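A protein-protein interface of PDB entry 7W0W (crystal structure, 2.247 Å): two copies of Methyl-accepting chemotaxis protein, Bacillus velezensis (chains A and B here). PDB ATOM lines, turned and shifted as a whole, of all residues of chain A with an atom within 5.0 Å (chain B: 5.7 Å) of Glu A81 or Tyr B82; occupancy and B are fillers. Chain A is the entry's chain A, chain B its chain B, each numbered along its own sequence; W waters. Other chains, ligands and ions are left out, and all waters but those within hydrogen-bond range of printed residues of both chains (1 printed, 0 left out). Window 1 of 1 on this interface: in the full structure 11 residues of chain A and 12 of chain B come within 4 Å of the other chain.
The side-chain carboxylate of Asp A77 lies within salt-bridge range of the side-chain amino group of Lys B78. NZ of Lys A78 is in salt-bridge range of OE1 of Glu B81 (3.3 Å). NZ of Lys B78 lies within salt-bridge range of OE1 of Glu A81, at 3.7 Å. OE1 of Glu A81 lies close to OE1 of Glu B81.
NZ of Lys B78 sits at hydrogen-bond distance from OH of Tyr B57 (3.0 Å). ND2 of Asn B86 lies within hydrogen-bond range of O of Tyr B82 (2.9 Å).
Among the printed residues, pairs that only touch across the chains: Lys A78 with Asp B77, Glu A81 with Tyr B57, Glu A81 with Phe B58, Glu A81 with Tyr B82, Tyr A82 with Glu B81, Tyr A82 with Ile B85, Lys A84 with Tyr B57, Ile A85 with Gly B54, Ile A85 with Tyr B57 and Ile A85 with Tyr B82.
Printed residues of chain B within 4 Å of Lys A78: Asp B77 (3.8 Å) and Glu B81 (2.8 Å). Glu A81 touches just these residues of chain B: Tyr B57 (3.6 Å), Phe B58 (3.9 Å), Lys B78 (2.9 Å), Glu B81 (3.2 Å) and Tyr B82 (3.6 Å). Of the printed residues of chain A, Tyr B57 touches Glu A81, Lys A84 and Ile A85. Tyr B82 touches just these residues of chain A: Glu A81 and Ile A85. Ile B92 touches none of the printed residues of chain A. The nearest residue of chain B that does not touch Glu A81 is Phe B79 (5.1 Å).
Of the 10 printed residues of chain A, 6 touch a printed residue of chain B. Along chain A the printed residues that touch a printed residue of chain B span positions 77 to 85. Hydrophobic or aromatic side chains of chain B that line the printed part of chain A: Tyr B57, Phe B58, Tyr B82 and Ile B85.
Asp A77 touches Lys B78, and with the chains exchanged Lys A78 touches Asp B77. Glu B81 touches its own counterpart, Glu A81. Glu A81 touches Tyr B82, and with the chains exchanged Tyr A82 touches Glu B81. Tyr A82 touches Ile B85, and with the chains exchanged Ile A85 touches Tyr B82.
Water W1 bridges OH of Tyr B57 (2.7 Å) and OD1 of Asp A77 (2.9 Å).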
ATOM      1  N   THR A  76      25.924  -1.400  33.729  1.00  0.00           N
ATOM      2  CA  THR A  76      27.056  -2.160  33.147  1.00  0.00           C
ATOM      3  C   THR A  76      26.602  -2.852  31.845  1.00  0.00           C
ATOM      4  O   THR A  76      27.353  -2.818  30.839  1.00  0.00           O
ATOM      5  CB  THR A  76      27.577  -3.203  34.145  1.00  0.00           C
ATOM      6  OG1 THR A  76      28.039  -2.542  35.318  1.00  0.00           O
ATOM      7  CG2 THR A  76      28.712  -4.021  33.592  1.00  0.00           C
ATOM      8  N   ASP A  77      25.425  -3.477  31.866  1.00  0.00           N
ATOM      9  CA  ASP A  77      24.883  -4.222  30.706  1.00  0.00           C
ATOM     10  C   ASP A  77      24.660  -3.224  29.567  1.00  0.00           C
ATOM     11  O   ASP A  77      25.068  -3.535  28.458  1.00  0.00           O
ATOM     12  CB  ASP A  77      23.625  -5.002  31.087  1.00  0.00           C
ATOM     13  CG  ASP A  77      23.087  -5.869  29.962  1.00  0.00           C
ATOM     14  OD1 ASP A  77      23.919  -6.519  29.243  1.00  0.00           O
ATOM     15  OD2 ASP A  77      21.836  -5.881  29.791  1.00  0.00           O
ATOM     16  N   LYS A  78      24.060  -2.063  29.834  1.00  0.00           N
ATOM     17  CA  LYS A  78      23.785  -1.065  28.778  1.00  0.00           C
ATOM     18  C   LYS A  78      25.101  -0.485  28.246  1.00  0.00           C
ATOM     19  O   LYS A  78      25.168  -0.270  27.032  1.00  0.00           O
ATOM     20  CB  LYS A  78      22.821   0.011  29.278  1.00  0.00           C
ATOM     21  CG  LYS A  78      21.364  -0.437  29.367  1.00  0.00           C
ATOM     22  CD  LYS A  78      20.446   0.751  29.480  1.00  0.00           C
ATOM     23  CE  LYS A  78      18.974   0.432  29.354  1.00  0.00           C
ATOM     24  NZ  LYS A  78      18.685  -0.335  28.119  1.00  0.00           N
ATOM     25  N   PHE A  79      26.100  -0.255  29.105  1.00  0.00           N
ATOM     26  CA  PHE A  79      27.433   0.255  28.711  1.00  0.00           C
ATOM     27  C   PHE A  79      28.156  -0.808  27.887  1.00  0.00           C
ATOM     28  O   PHE A  79      28.815  -0.454  26.899  1.00  0.00           O
ATOM     29  CB  PHE A  79      28.281   0.662  29.918  1.00  0.00           C
ATOM     30  CG  PHE A  79      27.925   1.980  30.564  1.00  0.00           C
ATOM     31  CD1 PHE A  79      26.828   2.724  30.157  1.00  0.00           C
ATOM     32  CD2 PHE A  79      28.700   2.476  31.603  1.00  0.00           C
ATOM     33  CE1 PHE A  79      26.544   3.954  30.746  1.00  0.00           C
ATOM     34  CE2 PHE A  79      28.405   3.695  32.197  1.00  0.00           C
ATOM     35  CZ  PHE A  79      27.308   4.412  31.793  1.00  0.00           C
ATOM     36  N   THR A  80      28.038  -2.071  28.263  1.00  0.00           N
ATOM     37  CA  THR A  80      28.684  -3.190  27.526  1.00  0.00           C
ATOM     38  C   THR A  80      28.124  -3.190  26.105  1.00  0.00           C
ATOM     39  O   THR A  80      28.933  -3.100  25.146  1.00  0.00           O
ATOM     40  CB  THR A  80      28.510  -4.525  28.257  1.00  0.00           C
ATOM     41  OG1 THR A  80      29.073  -4.293  29.545  1.00  0.00           O
ATOM     42  CG2 THR A  80      29.196  -5.689  27.578  1.00  0.00           C
ATOM     43  N   GLU A  81      26.797  -3.184  25.975  1.00  0.00           N
ATOM     44  CA  GLU A  81      26.123  -3.105  24.650  1.00  0.00           C
ATOM     45  C   GLU A  81      26.672  -1.907  23.845  1.00  0.00           C
ATOM     46  O   GLU A  81      27.048  -2.082  22.681  1.00  0.00           O
ATOM     47  CB  GLU A  81      24.601  -3.008  24.808  1.00  0.00           C
ATOM     48  CG  GLU A  81      23.901  -2.629  23.499  1.00  0.00           C
ATOM     49  CD  GLU A  81      22.389  -2.516  23.526  1.00  0.00           C
ATOM     50  OE1 GLU A  81      21.808  -2.918  24.500  1.00  0.00           O
ATOM     51  OE2 GLU A  81      21.799  -2.011  22.550  1.00  0.00           O
ATOM     52  N   TYR A  82      26.650  -0.707  24.418  1.00  0.00           N
ATOM     53  CA  TYR A  82      27.095   0.531  23.736  1.00  0.00           C
ATOM     54  C   TYR A  82      28.527   0.372  23.197  1.00  0.00           C
ATOM     55  O   TYR A  82      28.788   0.695  22.014  1.00  0.00           O
ATOM     56  CB  TYR A  82      26.992   1.734  24.676  1.00  0.00           C
ATOM     57  CG  TYR A  82      27.360   2.991  23.947  1.00  0.00           C
ATOM     58  CD1 TYR A  82      26.410   3.634  23.172  1.00  0.00           C
ATOM     59  CD2 TYR A  82      28.669   3.440  23.898  1.00  0.00           C
ATOM     60  CE1 TYR A  82      26.727   4.757  22.442  1.00  0.00           C
ATOM     61  CE2 TYR A  82      29.003   4.571  23.169  1.00  0.00           C
ATOM     62  CZ  TYR A  82      28.033   5.217  22.424  1.00  0.00           C
ATOM     63  OH  TYR A  82      28.325   6.322  21.682  1.00  0.00           O
ATOM     64  N   MET A  83      29.449  -0.111  24.024  1.00  0.00           N
ATOM     65  CA  MET A  83      30.889  -0.212  23.654  1.00  0.00           C
ATOM     66  C   MET A  83      31.085  -1.239  22.526  1.00  0.00           C
ATOM     67  O   MET A  83      31.840  -0.964  21.564  1.00  0.00           O
ATOM     68  CB  MET A  83      31.724  -0.635  24.869  1.00  0.00           C
ATOM     69  CG  MET A  83      33.227  -0.416  24.699  1.00  0.00           C
ATOM     70  SD  MET A  83      33.770   1.323  24.787  1.00  0.00           S
ATOM     71  CE  MET A  83      32.258   2.166  25.232  1.00  0.00           C
ATOM     72  N   LYS A  84      30.440  -2.392  22.650  1.00  0.00           N
ATOM     73  CA  LYS A  84      30.608  -3.517  21.702  1.00  0.00           C
ATOM     74  C   LYS A  84      30.078  -3.128  20.319  1.00  0.00           C
ATOM     75  O   LYS A  84      30.668  -3.605  19.364  1.00  0.00           O
ATOM     76  CB  LYS A  84      30.012  -4.800  22.289  1.00  0.00           C
ATOM     77  CG  LYS A  84      31.019  -5.521  23.161  1.00  0.00           C
ATOM     78  CD  LYS A  84      30.515  -6.727  23.863  1.00  0.00           C
ATOM     79  CE  LYS A  84      31.648  -7.468  24.536  1.00  0.00           C
ATOM     80  NZ  LYS A  84      31.128  -8.432  25.536  1.00  0.00           N
ATOM     81  N   ILE A  85      29.056  -2.273  20.229  1.00  0.00           N
ATOM     82  CA  ILE A  85      28.499  -1.747  18.948  1.00  0.00           C
ATOM     83  C   ILE A  85      29.414  -0.642  18.401  1.00  0.00           C
ATOM     84  O   ILE A  85      29.473  -0.503  17.180  1.00  0.00           O
ATOM     85  CB  ILE A  85      27.081  -1.160  19.130  1.00  0.00           C
ATOM     86  CG1 ILE A  85      26.111  -2.071  19.878  1.00  0.00           C
ATOM     87  CG2 ILE A  85      26.502  -0.733  17.804  1.00  0.00           C
ATOM     88  CD1 ILE A  85      25.738  -3.287  19.140  1.00  0.00           C
ATOM     89  N   GLN B  50      28.715  -0.006  10.198  1.00  0.00           N
ATOM     90  CA  GLN B  50      28.298   0.266  11.598  1.00  0.00           C
ATOM     91  C   GLN B  50      27.132  -0.658  11.948  1.00  0.00           C
ATOM     92  O   GLN B  50      27.158  -1.213  13.046  1.00  0.00           O
ATOM     93  CB  GLN B  50      27.952   1.736  11.811  1.00  0.00           C
ATOM     94  CG  GLN B  50      29.185   2.623  11.808  1.00  0.00           C
ATOM     95  CD  GLN B  50      28.884   4.105  11.737  1.00  0.00           C
ATOM     96  OE1 GLN B  50      27.750   4.535  11.514  1.00  0.00           O
ATOM     97  NE2 GLN B  50      29.933   4.900  11.878  1.00  0.00           N
ATOM     98  N   LYS B  51      26.186  -0.862  11.033  1.00  0.00           N
ATOM     99  CA  LYS B  51      25.040  -1.780  11.281  1.00  0.00           C
ATOM    100  C   LYS B  51      25.561  -3.212  11.469  1.00  0.00           C
ATOM    101  O   LYS B  51      25.016  -3.955  12.321  1.00  0.00           O
ATOM    102  CB  LYS B  51      23.974  -1.638  10.190  1.00  0.00           C
ATOM    103  CG  LYS B  51      23.347  -0.251  10.055  1.00  0.00           C
ATOM    104  CD  LYS B  51      23.534   0.658  11.260  1.00  0.00           C
ATOM    105  CE  LYS B  51      23.062   2.079  11.026  1.00  0.00           C
ATOM    106  NZ  LYS B  51      24.146   2.995  10.602  1.00  0.00           N
ATOM    107  N   GLY B  54      26.342  -3.824  14.930  1.00  0.00           N
ATOM    108  CA  GLY B  54      25.093  -4.144  15.669  1.00  0.00           C
ATOM    109  C   GLY B  54      24.698  -5.614  15.550  1.00  0.00           C
ATOM    110  O   GLY B  54      24.514  -6.265  16.585  1.00  0.00           O
ATOM    111  N   TYR B  57      27.139  -7.985  17.483  1.00  0.00           N
ATOM    112  CA  TYR B  57      26.820  -7.974  18.932  1.00  0.00           C
ATOM    113  C   TYR B  57      25.593  -8.849  19.209  1.00  0.00           C
ATOM    114  O   TYR B  57      25.651  -9.697  20.113  1.00  0.00           O
ATOM    115  CB  TYR B  57      26.510  -6.554  19.429  1.00  0.00           C
ATOM    116  CG  TYR B  57      26.033  -6.531  20.862  1.00  0.00           C
ATOM    117  CD1 TYR B  57      26.890  -6.878  21.894  1.00  0.00           C
ATOM    118  CD2 TYR B  57      24.724  -6.244  21.188  1.00  0.00           C
ATOM    119  CE1 TYR B  57      26.478  -6.889  23.215  1.00  0.00           C
ATOM    120  CE2 TYR B  57      24.292  -6.246  22.507  1.00  0.00           C
ATOM    121  CZ  TYR B  57      25.171  -6.567  23.530  1.00  0.00           C
ATOM    122  OH  TYR B  57      24.738  -6.567  24.826  1.00  0.00           O
ATOM    123  N   PHE B  58      24.475  -8.602  18.518  1.00  0.00           N
ATOM    124  CA  PHE B  58      23.205  -9.347  18.777  1.00  0.00           C
ATOM    125  C   PHE B  58      23.363 -10.832  18.390  1.00  0.00           C
ATOM    126  O   PHE B  58      22.768 -11.648  19.085  1.00  0.00           O
ATOM    127  CB  PHE B  58      22.027  -8.630  18.123  1.00  0.00           C
ATOM    128  CG  PHE B  58      21.606  -7.414  18.897  1.00  0.00           C
ATOM    129  CD1 PHE B  58      20.995  -7.549  20.133  1.00  0.00           C
ATOM    130  CD2 PHE B  58      21.864  -6.136  18.420  1.00  0.00           C
ATOM    131  CE1 PHE B  58      20.596  -6.428  20.851  1.00  0.00           C
ATOM    132  CE2 PHE B  58      21.488  -5.016  19.144  1.00  0.00           C
ATOM    133  CZ  PHE B  58      20.861  -5.160  20.362  1.00  0.00           C
ATOM    134  N   ASP B  77      14.305  -4.234  25.512  1.00  0.00           N
ATOM    135  CA  ASP B  77      15.128  -3.217  26.208  1.00  0.00           C
ATOM    136  C   ASP B  77      16.408  -2.970  25.393  1.00  0.00           C
ATOM    137  O   ASP B  77      16.745  -1.792  25.174  1.00  0.00           O
ATOM    138  CB  ASP B  77      15.426  -3.614  27.660  1.00  0.00           C
ATOM    139  CG  ASP B  77      14.215  -3.647  28.597  1.00  0.00           C
ATOM    140  OD1 ASP B  77      13.174  -3.005  28.266  1.00  0.00           O
ATOM    141  OD2 ASP B  77      14.321  -4.310  29.668  1.00  0.00           O
ATOM    142  N   LYS B  78      17.099  -4.018  24.958  1.00  0.00           N
ATOM    143  CA  LYS B  78      18.364  -3.858  24.197  1.00  0.00           C
ATOM    144  C   LYS B  78      18.088  -3.249  22.813  1.00  0.00           C
ATOM    145  O   LYS B  78      18.917  -2.432  22.372  1.00  0.00           O
ATOM    146  CB  LYS B  78      19.098  -5.192  24.093  1.00  0.00           C
ATOM    147  CG  LYS B  78      19.828  -5.615  25.356  1.00  0.00           C
ATOM    148  CD  LYS B  78      20.865  -6.673  25.054  1.00  0.00           C
ATOM    149  CE  LYS B  78      21.742  -6.994  26.235  1.00  0.00           C
ATOM    150  NZ  LYS B  78      22.488  -5.798  26.679  1.00  0.00           N
ATOM    151  N   PHE B  79      16.978  -3.624  22.158  1.00  0.00           N
ATOM    152  CA  PHE B  79      16.553  -3.057  20.847  1.00  0.00           C
ATOM    153  C   PHE B  79      16.172  -1.584  21.032  1.00  0.00           C
ATOM    154  O   PHE B  79      16.517  -0.771  20.166  1.00  0.00           O
ATOM    155  CB  PHE B  79      15.389  -3.831  20.235  1.00  0.00           C
ATOM    156  CG  PHE B  79      15.739  -5.164  19.611  1.00  0.00           C
ATOM    157  CD1 PHE B  79      17.015  -5.694  19.674  1.00  0.00           C
ATOM    158  CD2 PHE B  79      14.764  -5.895  18.942  1.00  0.00           C
ATOM    159  CE1 PHE B  79      17.308  -6.901  19.045  1.00  0.00           C
ATOM    160  CE2 PHE B  79      15.052  -7.107  18.334  1.00  0.00           C
ATOM    161  CZ  PHE B  79      16.317  -7.623  18.396  1.00  0.00           C
ATOM    162  N   THR B  80      15.506  -1.235  22.130  1.00  0.00           N
ATOM    163  CA  THR B  80      15.129   0.173  22.434  1.00  0.00           C
ATOM    164  C   THR B  80      16.411   1.000  22.492  1.00  0.00           C
ATOM    165  O   THR B  80      16.523   1.993  21.757  1.00  0.00           O
ATOM    166  CB  THR B  80      14.302   0.269  23.722  1.00  0.00           C
ATOM    167  OG1 THR B  80      13.176  -0.556  23.459  1.00  0.00           O
ATOM    168  CG2 THR B  80      13.834   1.669  24.052  1.00  0.00           C
ATOM    169  N   GLU B  81      17.383   0.555  23.279  1.00  0.00           N
ATOM    170  CA  GLU B  81      18.690   1.241  23.398  1.00  0.00           C
ATOM    171  C   GLU B  81      19.318   1.439  22.007  1.00  0.00           C
ATOM    172  O   GLU B  81      19.730   2.571  21.682  1.00  0.00           O
ATOM    173  CB  GLU B  81      19.631   0.428  24.283  1.00  0.00           C
ATOM    174  CG  GLU B  81      21.068   0.949  24.244  1.00  0.00           C
ATOM    175  CD  GLU B  81      21.991   0.334  25.288  1.00  0.00           C
ATOM    176  OE1 GLU B  81      21.477  -0.220  26.277  1.00  0.00           O
ATOM    177  OE2 GLU B  81      23.216   0.420  25.114  1.00  0.00           O
ATOM    178  N   TYR B  82      19.445   0.359  21.234  1.00  0.00           N
ATOM    179  CA  TYR B  82      20.055   0.365  19.893  1.00  0.00           C
ATOM    180  C   TYR B  82      19.381   1.439  19.022  1.00  0.00           C
ATOM    181  O   TYR B  82      20.085   2.252  18.403  1.00  0.00           O
ATOM    182  CB  TYR B  82      19.960  -1.015  19.236  1.00  0.00           C
ATOM    183  CG  TYR B  82      20.677  -1.004  17.919  1.00  0.00           C
ATOM    184  CD1 TYR B  82      22.041  -1.164  17.902  1.00  0.00           C
ATOM    185  CD2 TYR B  82      20.038  -0.656  16.737  1.00  0.00           C
ATOM    186  CE1 TYR B  82      22.767  -1.053  16.733  1.00  0.00           C
ATOM    187  CE2 TYR B  82      20.758  -0.529  15.559  1.00  0.00           C
ATOM    188  CZ  TYR B  82      22.128  -0.727  15.560  1.00  0.00           C
ATOM    189  OH  TYR B  82      22.897  -0.641  14.439  1.00  0.00           O
ATOM    190  N   MET B  83      18.053   1.446  18.963  1.00  0.00           N
ATOM    191  CA  MET B  83      17.287   2.344  18.060  1.00  0.00           C
ATOM    192  C   MET B  83      17.448   3.806  18.492  1.00  0.00           C
ATOM    193  O   MET B  83      17.654   4.679  17.631  1.00  0.00           O
ATOM    194  CB  MET B  83      15.805   1.969  18.072  1.00  0.00           C
ATOM    195  CG  MET B  83      15.466   1.010  16.941  1.00  0.00           C
ATOM    196  SD  MET B  83      15.164   1.864  15.383  1.00  0.00           S
ATOM    197  CE  MET B  83      14.263   3.328  15.889  1.00  0.00           C
ATOM    198  N   LYS B  84      17.344   4.073  19.788  1.00  0.00           N
ATOM    199  CA  LYS B  84      17.356   5.458  20.302  1.00  0.00           C
ATOM    200  C   LYS B  84      18.749   6.062  20.103  1.00  0.00           C
ATOM    201  O   LYS B  84      18.793   7.254  19.853  1.00  0.00           O
ATOM    202  CB  LYS B  84      16.877   5.491  21.751  1.00  0.00           C
ATOM    203  CG  LYS B  84      15.367   5.533  21.933  1.00  0.00           C
ATOM    204  CD  LYS B  84      15.041   5.492  23.407  1.00  0.00           C
ATOM    205  CE  LYS B  84      13.619   5.804  23.787  1.00  0.00           C
ATOM    206  NZ  LYS B  84      12.706   5.238  22.784  1.00  0.00           N
ATOM    207  N   ILE B  85      19.837   5.282  20.140  1.00  0.00           N
ATOM    208  CA  ILE B  85      21.201   5.846  19.877  1.00  0.00           C
ATOM    209  C   ILE B  85      21.460   5.888  18.367  1.00  0.00           C
ATOM    210  O   ILE B  85      22.290   6.713  17.986  1.00  0.00           O
ATOM    211  CB  ILE B  85      22.338   5.122  20.630  1.00  0.00           C
ATOM    212  CG1 ILE B  85      22.603   3.736  20.034  1.00  0.00           C
ATOM    213  CG2 ILE B  85      22.058   5.088  22.130  1.00  0.00           C
ATOM    214  CD1 ILE B  85      23.536   2.832  20.824  1.00  0.00           C
ATOM    215  N   ASN B  86      20.832   5.042  17.536  1.00  0.00           N
ATOM    216  CA  ASN B  86      21.111   4.997  16.067  1.00  0.00           C
ATOM    217  C   ASN B  86      19.951   5.638  15.294  1.00  0.00           C
ATOM    218  O   ASN B  86      19.086   4.903  14.804  1.00  0.00           O
ATOM    219  CB  ASN B  86      21.406   3.583  15.576  1.00  0.00           C
ATOM    220  CG  ASN B  86      22.717   3.063  16.112  1.00  0.00           C
ATOM    221  OD1 ASN B  86      23.772   3.482  15.656  1.00  0.00           O
ATOM    222  ND2 ASN B  86      22.664   2.229  17.135  1.00  0.00           N
ATOM    223  N   VAL B  89      18.383   4.542  11.833  1.00  0.00           N
ATOM    224  CA  VAL B  89      17.841   3.152  11.694  1.00  0.00           C
ATOM    225  C   VAL B  89      16.311   3.174  11.626  1.00  0.00           C
ATOM    226  O   VAL B  89      15.693   3.879  12.426  1.00  0.00           O
ATOM    227  CB  VAL B  89      18.336   2.261  12.843  1.00  0.00           C
ATOM    228  CG1 VAL B  89      17.609   0.923  12.888  1.00  0.00           C
ATOM    229  CG2 VAL B  89      19.838   2.049  12.740  1.00  0.00           C
ATOM    230  N   ILE B  92      14.906  -2.554  14.196  1.00  0.00           N
ATOM    231  CA  ILE B  92      15.728  -3.746  14.489  1.00  0.00           C
ATOM    232  C   ILE B  92      14.741  -4.828  14.921  1.00  0.00           C
ATOM    233  O   ILE B  92      13.736  -4.496  15.630  1.00  0.00           O
ATOM    234  CB  ILE B  92      16.834  -3.438  15.525  1.00  0.00           C
ATOM    235  CG1 ILE B  92      17.688  -4.668  15.827  1.00  0.00           C
ATOM    236  CG2 ILE B  92      16.284  -2.860  16.817  1.00  0.00           C
ATOM    237  CD1 ILE B  92      18.934  -4.332  16.625  1.00  0.00           C
ATOM    238  N   ILE B 162      18.650  -5.374  10.900  1.00  0.00           N
ATOM    239  CA  ILE B 162      18.570  -3.893  11.061  1.00  0.00           C
ATOM    240  C   ILE B 162      18.192  -3.294   9.700  1.00  0.00           C
ATOM    241  O   ILE B 162      18.872  -3.610   8.713  1.00  0.00           O
ATOM    242  CB  ILE B 162      19.903  -3.329  11.585  1.00  0.00           C
ATOM    243  CG1 ILE B 162      20.280  -3.940  12.941  1.00  0.00           C
ATOM    244  CG2 ILE B 162      19.855  -1.815  11.661  1.00  0.00           C
ATOM    245  CD1 ILE B 162      21.639  -3.509  13.451  1.00  0.00           C
HETATM  246  O   HOH W   1      25.814  -7.319  27.237  1.00  0.00           O
